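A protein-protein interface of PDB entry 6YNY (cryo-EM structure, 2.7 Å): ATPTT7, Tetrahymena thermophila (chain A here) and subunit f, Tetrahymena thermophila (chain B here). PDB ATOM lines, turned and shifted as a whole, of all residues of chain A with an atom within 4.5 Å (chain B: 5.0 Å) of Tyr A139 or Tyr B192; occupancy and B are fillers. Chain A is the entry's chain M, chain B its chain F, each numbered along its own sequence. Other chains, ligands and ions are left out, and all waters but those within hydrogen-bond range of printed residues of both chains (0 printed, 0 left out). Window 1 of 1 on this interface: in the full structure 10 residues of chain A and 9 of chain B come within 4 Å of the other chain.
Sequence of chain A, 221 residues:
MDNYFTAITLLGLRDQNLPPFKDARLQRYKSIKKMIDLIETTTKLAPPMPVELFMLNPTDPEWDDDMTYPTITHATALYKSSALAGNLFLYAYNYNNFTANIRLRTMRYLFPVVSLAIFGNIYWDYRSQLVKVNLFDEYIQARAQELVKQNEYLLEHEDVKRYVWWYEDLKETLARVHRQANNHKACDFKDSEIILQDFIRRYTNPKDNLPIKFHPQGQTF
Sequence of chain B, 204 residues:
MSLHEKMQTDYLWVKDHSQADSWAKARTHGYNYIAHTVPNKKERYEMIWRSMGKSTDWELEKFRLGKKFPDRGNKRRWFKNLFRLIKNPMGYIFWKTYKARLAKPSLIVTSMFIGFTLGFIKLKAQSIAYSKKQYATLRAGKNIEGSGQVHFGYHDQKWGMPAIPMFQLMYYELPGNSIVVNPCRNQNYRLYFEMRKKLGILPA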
ATOM      1  N   MET A  67      36.110  11.300   6.409  1.00  0.00           N
ATOM      2  CA  MET A  67      35.688  12.052   7.575  1.00  0.00           C
ATOM      3  C   MET A  67      36.348  11.521   8.842  1.00  0.00           C
ATOM      4  O   MET A  67      36.676  10.338   8.954  1.00  0.00           O
ATOM      5  CB  MET A  67      34.171  11.992   7.715  1.00  0.00           C
ATOM      6  CG  MET A  67      33.626  12.861   8.808  1.00  0.00           C
ATOM      7  SD  MET A  67      34.085  14.581   8.598  1.00  0.00           S
ATOM      8  CE  MET A  67      33.435  15.245  10.110  1.00  0.00           C
ATOM      9  N   LEU A 135      25.672  16.144  15.674  1.00  0.00           N
ATOM     10  CA  LEU A 135      25.419  16.139  14.238  1.00  0.00           C
ATOM     11  C   LEU A 135      25.952  14.871  13.592  1.00  0.00           C
ATOM     12  O   LEU A 135      25.361  14.362  12.633  1.00  0.00           O
ATOM     13  CB  LEU A 135      26.060  17.362  13.586  1.00  0.00           C
ATOM     14  CG  LEU A 135      25.505  18.730  13.960  1.00  0.00           C
ATOM     15  CD1 LEU A 135      26.312  19.799  13.284  1.00  0.00           C
ATOM     16  CD2 LEU A 135      24.057  18.849  13.570  1.00  0.00           C
ATOM     17  N   PHE A 136      27.067  14.351  14.100  1.00  0.00           N
ATOM     18  CA  PHE A 136      27.653  13.141  13.544  1.00  0.00           C
ATOM     19  C   PHE A 136      26.838  11.915  13.922  1.00  0.00           C
ATOM     20  O   PHE A 136      26.595  11.041  13.082  1.00  0.00           O
ATOM     21  CB  PHE A 136      29.091  13.013  14.035  1.00  0.00           C
ATOM     22  CG  PHE A 136      29.801  11.797  13.540  1.00  0.00           C
ATOM     23  CD1 PHE A 136      30.442  11.807  12.321  1.00  0.00           C
ATOM     24  CD2 PHE A 136      29.846  10.649  14.303  1.00  0.00           C
ATOM     25  CE1 PHE A 136      31.101  10.691  11.871  1.00  0.00           C
ATOM     26  CE2 PHE A 136      30.501   9.539  13.857  1.00  0.00           C
ATOM     27  CZ  PHE A 136      31.132   9.557  12.640  1.00  0.00           C
ATOM     28  N   ASP A 137      26.403  11.836  15.179  1.00  0.00           N
ATOM     29  CA  ASP A 137      25.644  10.675  15.624  1.00  0.00           C
ATOM     30  C   ASP A 137      24.304  10.582  14.908  1.00  0.00           C
ATOM     31  O   ASP A 137      23.865   9.485  14.544  1.00  0.00           O
ATOM     32  CB  ASP A 137      25.441  10.733  17.136  1.00  0.00           C
ATOM     33  CG  ASP A 137      26.745  10.656  17.907  1.00  0.00           C
ATOM     34  OD1 ASP A 137      27.760  10.222  17.323  1.00  0.00           O
ATOM     35  OD2 ASP A 137      26.755  11.020  19.101  1.00  0.00           O
ATOM     36  N   GLU A 138      23.635  11.715  14.698  1.00  0.00           N
ATOM     37  CA  GLU A 138      22.322  11.697  14.070  1.00  0.00           C
ATOM     38  C   GLU A 138      22.389  11.463  12.568  1.00  0.00           C
ATOM     39  O   GLU A 138      21.382  11.071  11.973  1.00  0.00           O
ATOM     40  CB  GLU A 138      21.580  13.005  14.353  1.00  0.00           C
ATOM     41  CG  GLU A 138      22.151  14.220  13.662  1.00  0.00           C
ATOM     42  CD  GLU A 138      21.407  15.490  14.019  1.00  0.00           C
ATOM     43  OE1 GLU A 138      20.449  15.414  14.817  1.00  0.00           O
ATOM     44  OE2 GLU A 138      21.777  16.564  13.502  1.00  0.00           O
ATOM     45  N   TYR A 139      23.545  11.694  11.944  1.00  0.00           N
ATOM     46  CA  TYR A 139      23.668  11.482  10.508  1.00  0.00           C
ATOM     47  C   TYR A 139      23.939  10.022  10.179  1.00  0.00           C
ATOM     48  O   TYR A 139      23.341   9.469   9.251  1.00  0.00           O
ATOM     49  CB  TYR A 139      24.778  12.367   9.943  1.00  0.00           C
ATOM     50  CG  TYR A 139      25.001  12.190   8.462  1.00  0.00           C
ATOM     51  CD1 TYR A 139      24.179  12.815   7.542  1.00  0.00           C
ATOM     52  CD2 TYR A 139      26.032  11.401   7.983  1.00  0.00           C
ATOM     53  CE1 TYR A 139      24.373  12.658   6.198  1.00  0.00           C
ATOM     54  CE2 TYR A 139      26.233  11.240   6.637  1.00  0.00           C
ATOM     55  CZ  TYR A 139      25.401  11.870   5.748  1.00  0.00           C
ATOM     56  OH  TYR A 139      25.599  11.711   4.401  1.00  0.00           O
ATOM     57  N   ILE A 140      24.841   9.386  10.925  1.00  0.00           N
ATOM     58  CA  ILE A 140      25.172   7.990  10.670  1.00  0.00           C
ATOM     59  C   ILE A 140      23.960   7.100  10.882  1.00  0.00           C
ATOM     60  O   ILE A 140      23.835   6.045  10.250  1.00  0.00           O
ATOM     61  CB  ILE A 140      26.349   7.561  11.563  1.00  0.00           C
ATOM     62  CG1 ILE A 140      25.978   7.712  13.034  1.00  0.00           C
ATOM     63  CG2 ILE A 140      27.571   8.396  11.247  1.00  0.00           C
ATOM     64  CD1 ILE A 140      26.998   7.161  13.962  1.00  0.00           C
ATOM     65  N   GLN A 141      23.054   7.496  11.775  1.00  0.00           N
ATOM     66  CA  GLN A 141      21.850   6.713  12.011  1.00  0.00           C
ATOM     67  C   GLN A 141      20.825   6.920  10.907  1.00  0.00           C
ATOM     68  O   GLN A 141      20.167   5.965  10.482  1.00  0.00           O
ATOM     69  CB  GLN A 141      21.250   7.071  13.368  1.00  0.00           C
ATOM     70  CG  GLN A 141      22.056   6.566  14.545  1.00  0.00           C
ATOM     71  CD  GLN A 141      21.454   6.955  15.877  1.00  0.00           C
ATOM     72  OE1 GLN A 141      20.697   6.192  16.476  1.00  0.00           O
ATOM     73  NE2 GLN A 141      21.790   8.144  16.351  1.00  0.00           N
ATOM     74  N   ALA A 142      20.676   8.154  10.430  1.00  0.00           N
ATOM     75  CA  ALA A 142      19.725   8.419   9.358  1.00  0.00           C
ATOM     76  C   ALA A 142      20.215   7.840   8.037  1.00  0.00           C
ATOM     77  O   ALA A 142      19.448   7.204   7.305  1.00  0.00           O
ATOM     78  CB  ALA A 142      19.489   9.920   9.230  1.00  0.00           C
ATOM     79  N   ARG A 143      21.490   8.049   7.715  1.00  0.00           N
ATOM     80  CA  ARG A 143      22.027   7.543   6.461  1.00  0.00           C
ATOM     81  C   ARG A 143      22.107   6.025   6.452  1.00  0.00           C
ATOM     82  O   ARG A 143      22.089   5.421   5.376  1.00  0.00           O
ATOM     83  CB  ARG A 143      23.404   8.155   6.205  1.00  0.00           C
ATOM     84  CG  ARG A 143      24.083   7.703   4.932  1.00  0.00           C
ATOM     85  CD  ARG A 143      23.259   8.012   3.711  1.00  0.00           C
ATOM     86  NE  ARG A 143      23.875   7.506   2.493  1.00  0.00           N
ATOM     87  CZ  ARG A 143      23.217   7.291   1.362  1.00  0.00           C
ATOM     88  NH1 ARG A 143      21.919   7.531   1.286  1.00  0.00           N
ATOM     89  NH2 ARG A 143      23.860   6.828   0.303  1.00  0.00           N
ATOM     90  N   ASN B 188      32.466  18.375   5.153  1.00  0.00           N
ATOM     91  CA  ASN B 188      31.548  17.251   5.230  1.00  0.00           C
ATOM     92  C   ASN B 188      30.363  17.536   6.136  1.00  0.00           C
ATOM     93  O   ASN B 188      29.378  16.794   6.094  1.00  0.00           O
ATOM     94  CB  ASN B 188      32.287  16.009   5.715  1.00  0.00           C
ATOM     95  CG  ASN B 188      33.423  15.623   4.806  1.00  0.00           C
ATOM     96  OD1 ASN B 188      33.403  15.904   3.610  1.00  0.00           O
ATOM     97  ND2 ASN B 188      34.425  14.972   5.367  1.00  0.00           N
ATOM     98  N   TYR B 189      30.441  18.583   6.957  1.00  0.00           N
ATOM     99  CA  TYR B 189      29.307  18.987   7.772  1.00  0.00           C
ATOM    100  C   TYR B 189      28.169  19.538   6.930  1.00  0.00           C
ATOM    101  O   TYR B 189      27.039  19.627   7.418  1.00  0.00           O
ATOM    102  CB  TYR B 189      29.752  20.023   8.799  1.00  0.00           C
ATOM    103  CG  TYR B 189      30.516  19.436   9.955  1.00  0.00           C
ATOM    104  CD1 TYR B 189      31.859  19.132   9.840  1.00  0.00           C
ATOM    105  CD2 TYR B 189      29.892  19.185  11.162  1.00  0.00           C
ATOM    106  CE1 TYR B 189      32.555  18.593  10.890  1.00  0.00           C
ATOM    107  CE2 TYR B 189      30.579  18.646  12.219  1.00  0.00           C
ATOM    108  CZ  TYR B 189      31.911  18.351  12.081  1.00  0.00           C
ATOM    109  OH  TYR B 189      32.600  17.812  13.139  1.00  0.00           O
ATOM    110  N   ARG B 190      28.444  19.912   5.682  1.00  0.00           N
ATOM    111  CA  ARG B 190      27.380  20.346   4.788  1.00  0.00           C
ATOM    112  C   ARG B 190      26.343  19.248   4.599  1.00  0.00           C
ATOM    113  O   ARG B 190      25.146  19.529   4.473  1.00  0.00           O
ATOM    114  CB  ARG B 190      27.972  20.755   3.444  1.00  0.00           C
ATOM    115  CG  ARG B 190      29.048  21.811   3.537  1.00  0.00           C
ATOM    116  CD  ARG B 190      29.603  22.152   2.177  1.00  0.00           C
ATOM    117  NE  ARG B 190      30.627  23.185   2.239  1.00  0.00           N
ATOM    118  CZ  ARG B 190      31.020  23.906   1.198  1.00  0.00           C
ATOM    119  NH1 ARG B 190      30.473  23.722   0.010  1.00  0.00           N
ATOM    120  NH2 ARG B 190      31.958  24.822   1.347  1.00  0.00           N
ATOM    121  N   LEU B 191      26.785  17.991   4.576  1.00  0.00           N
ATOM    122  CA  LEU B 191      25.851  16.876   4.494  1.00  0.00           C
ATOM    123  C   LEU B 191      24.873  16.888   5.658  1.00  0.00           C
ATOM    124  O   LEU B 191      23.688  16.579   5.486  1.00  0.00           O
ATOM    125  CB  LEU B 191      26.621  15.560   4.473  1.00  0.00           C
ATOM    126  CG  LEU B 191      27.563  15.340   3.299  1.00  0.00           C
ATOM    127  CD1 LEU B 191      28.539  14.233   3.613  1.00  0.00           C
ATOM    128  CD2 LEU B 191      26.772  15.002   2.065  1.00  0.00           C
ATOM    129  N   TYR B 192      25.350  17.236   6.850  1.00  0.00           N
ATOM    130  CA  TYR B 192      24.483  17.228   8.021  1.00  0.00           C
ATOM    131  C   TYR B 192      23.429  18.321   7.930  1.00  0.00           C
ATOM    132  O   TYR B 192      22.259  18.091   8.256  1.00  0.00           O
ATOM    133  CB  TYR B 192      25.318  17.393   9.288  1.00  0.00           C
ATOM    134  CG  TYR B 192      26.470  16.425   9.410  1.00  0.00           C
ATOM    135  CD1 TYR B 192      27.552  16.707  10.222  1.00  0.00           C
ATOM    136  CD2 TYR B 192      26.474  15.230   8.716  1.00  0.00           C
ATOM    137  CE1 TYR B 192      28.602  15.831  10.338  1.00  0.00           C
ATOM    138  CE2 TYR B 192      27.521  14.349   8.824  1.00  0.00           C
ATOM    139  CZ  TYR B 192      28.582  14.653   9.636  1.00  0.00           C
ATOM    140  OH  TYR B 192      29.626  13.771   9.747  1.00  0.00           O
ATOM    141  N   PHE B 193      23.824  19.514   7.494  1.00  0.00           N
ATOM    142  CA  PHE B 193      22.877  20.613   7.378  1.00  0.00           C
ATOM    143  C   PHE B 193      21.816  20.331   6.327  1.00  0.00           C
ATOM    144  O   PHE B 193      20.671  20.773   6.468  1.00  0.00           O
ATOM    145  CB  PHE B 193      23.624  21.902   7.051  1.00  0.00           C
ATOM    146  CG  PHE B 193      24.714  22.228   8.022  1.00  0.00           C
ATOM    147  CD1 PHE B 193      24.548  21.997   9.372  1.00  0.00           C
ATOM    148  CD2 PHE B 193      25.912  22.751   7.586  1.00  0.00           C
ATOM    149  CE1 PHE B 193      25.546  22.291  10.260  1.00  0.00           C
ATOM    150  CE2 PHE B 193      26.915  23.046   8.476  1.00  0.00           C
ATOM    151  CZ  PHE B 193      26.731  22.815   9.813  1.00  0.00           C
ATOM    152  N   GLU B 194      22.172  19.602   5.272  1.00  0.00           N
ATOM    153  CA  GLU B 194      21.207  19.281   4.229  1.00  0.00           C
ATOM    154  C   GLU B 194      20.261  18.169   4.662  1.00  0.00           C
ATOM    155  O   GLU B 194      19.080  18.181   4.301  1.00  0.00           O
ATOM    156  CB  GLU B 194      21.943  18.893   2.951  1.00  0.00           C
ATOM    157  CG  GLU B 194      22.807  20.004   2.387  1.00  0.00           C
ATOM    158  CD  GLU B 194      23.714  19.532   1.270  1.00  0.00           C
ATOM    159  OE1 GLU B 194      23.568  18.374   0.829  1.00  0.00           O
ATOM    160  OE2 GLU B 194      24.578  20.320   0.834  1.00  0.00           O
ATOM    161  N   MET B 195      20.760  17.201   5.431  1.00  0.00           N
ATOM    162  CA  MET B 195      19.899  16.134   5.925  1.00  0.00           C
ATOM    163  C   MET B 195      18.899  16.663   6.943  1.00  0.00           C
ATOM    164  O   MET B 195      17.726  16.276   6.928  1.00  0.00           O
ATOM    165  CB  MET B 195      20.746  15.024   6.541  1.00  0.00           C
ATOM    166  CG  MET B 195      19.951  13.854   7.095  1.00  0.00           C
ATOM    167  SD  MET B 195      19.215  12.813   5.828  1.00  0.00           S
ATOM    168  CE  MET B 195      20.652  11.879   5.325  1.00  0.00           C
ATOM    169  N   ARG B 196      19.347  17.547   7.833  1.00  0.00           N
ATOM    170  CA  ARG B 196      18.452  18.098   8.843  1.00  0.00           C
ATOM    171  C   ARG B 196      17.263  18.799   8.204  1.00  0.00           C
ATOM    172  O   ARG B 196      16.145  18.741   8.726  1.00  0.00           O
ATOM    173  CB  ARG B 196      19.221  19.057   9.745  1.00  0.00           C
ATOM    174  CG  ARG B 196      20.224  18.368  10.634  1.00  0.00           C
ATOM    175  CD  ARG B 196      21.203  19.341  11.247  1.00  0.00           C
ATOM    176  NE  ARG B 196      20.549  20.356  12.065  1.00  0.00           N
ATOM    177  CZ  ARG B 196      20.215  20.194  13.340  1.00  0.00           C
ATOM    178  NH1 ARG B 196      19.625  21.179  13.995  1.00  0.00           N
ATOM    179  NH2 ARG B 196      20.458  19.052  13.959  1.00  0.00           N
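SD of Met A67 is in hydrogen-bond range of ND2 of Asn B188.
NH2 of Arg B196 is in salt-bridge range of OE2 of Glu A138 (2.9 Å).
Among the printed residues, pairs that only touch across the chains: Met A67 with Tyr B189 (3.5 Å), Leu A135 with Tyr B192 (3.7 Å), Leu A135 with Phe B193 (3.99 Å), Leu A135 with Arg B196 (3.6 Å), Phe A136 with Tyr B192 (3.3 Å), Tyr A139 with Leu B191 (3.95 Å), Tyr A139 with Tyr B192 (3.3 Å) and Tyr A139 with Met B195 (3.9 Å).
Of the printed residues of chain B, Leu A135 touches Tyr B192, Phe B193 and Arg B196.
Of chain B, only Leu B191, Tyr B192 and Met B195 come within 4 Å of Tyr A139.
Ile A140 touches none of the printed residues of chain B.
Printed residues of chain A within 4 Å of Asn B188: Met A67.
Printed residues of chain A within 4 Å of Tyr B189: Met A67.
Arg B190 touches none of the printed residues of chain A.
Of the printed residues of chain A, Leu B191 touches Tyr A139.
Of chain A, only Leu A135, Phe A136 and Tyr A139 come within 4 Å of Tyr B192.
Printed residues of chain A within 4 Å of Arg B196: Leu A135 and Glu A138.
Printed residues of chain A that touch a printed residue of chain B: Met A67, Leu A135, Phe A136, Glu A138 and Tyr A139.
Hydrophobic or aromatic side chains of chain A within 4 Å of the printed part of chain B: Met A67, Leu A135, Phe A136 and Tyr A139.
Of the 9 printed residues of chain B, 7 touch a printed residue of chain A.
Along chain B the printed residues that touch a printed residue of chain A span positions 188 to 196.
Among the printed residues, 10 pairs touch across the chains.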
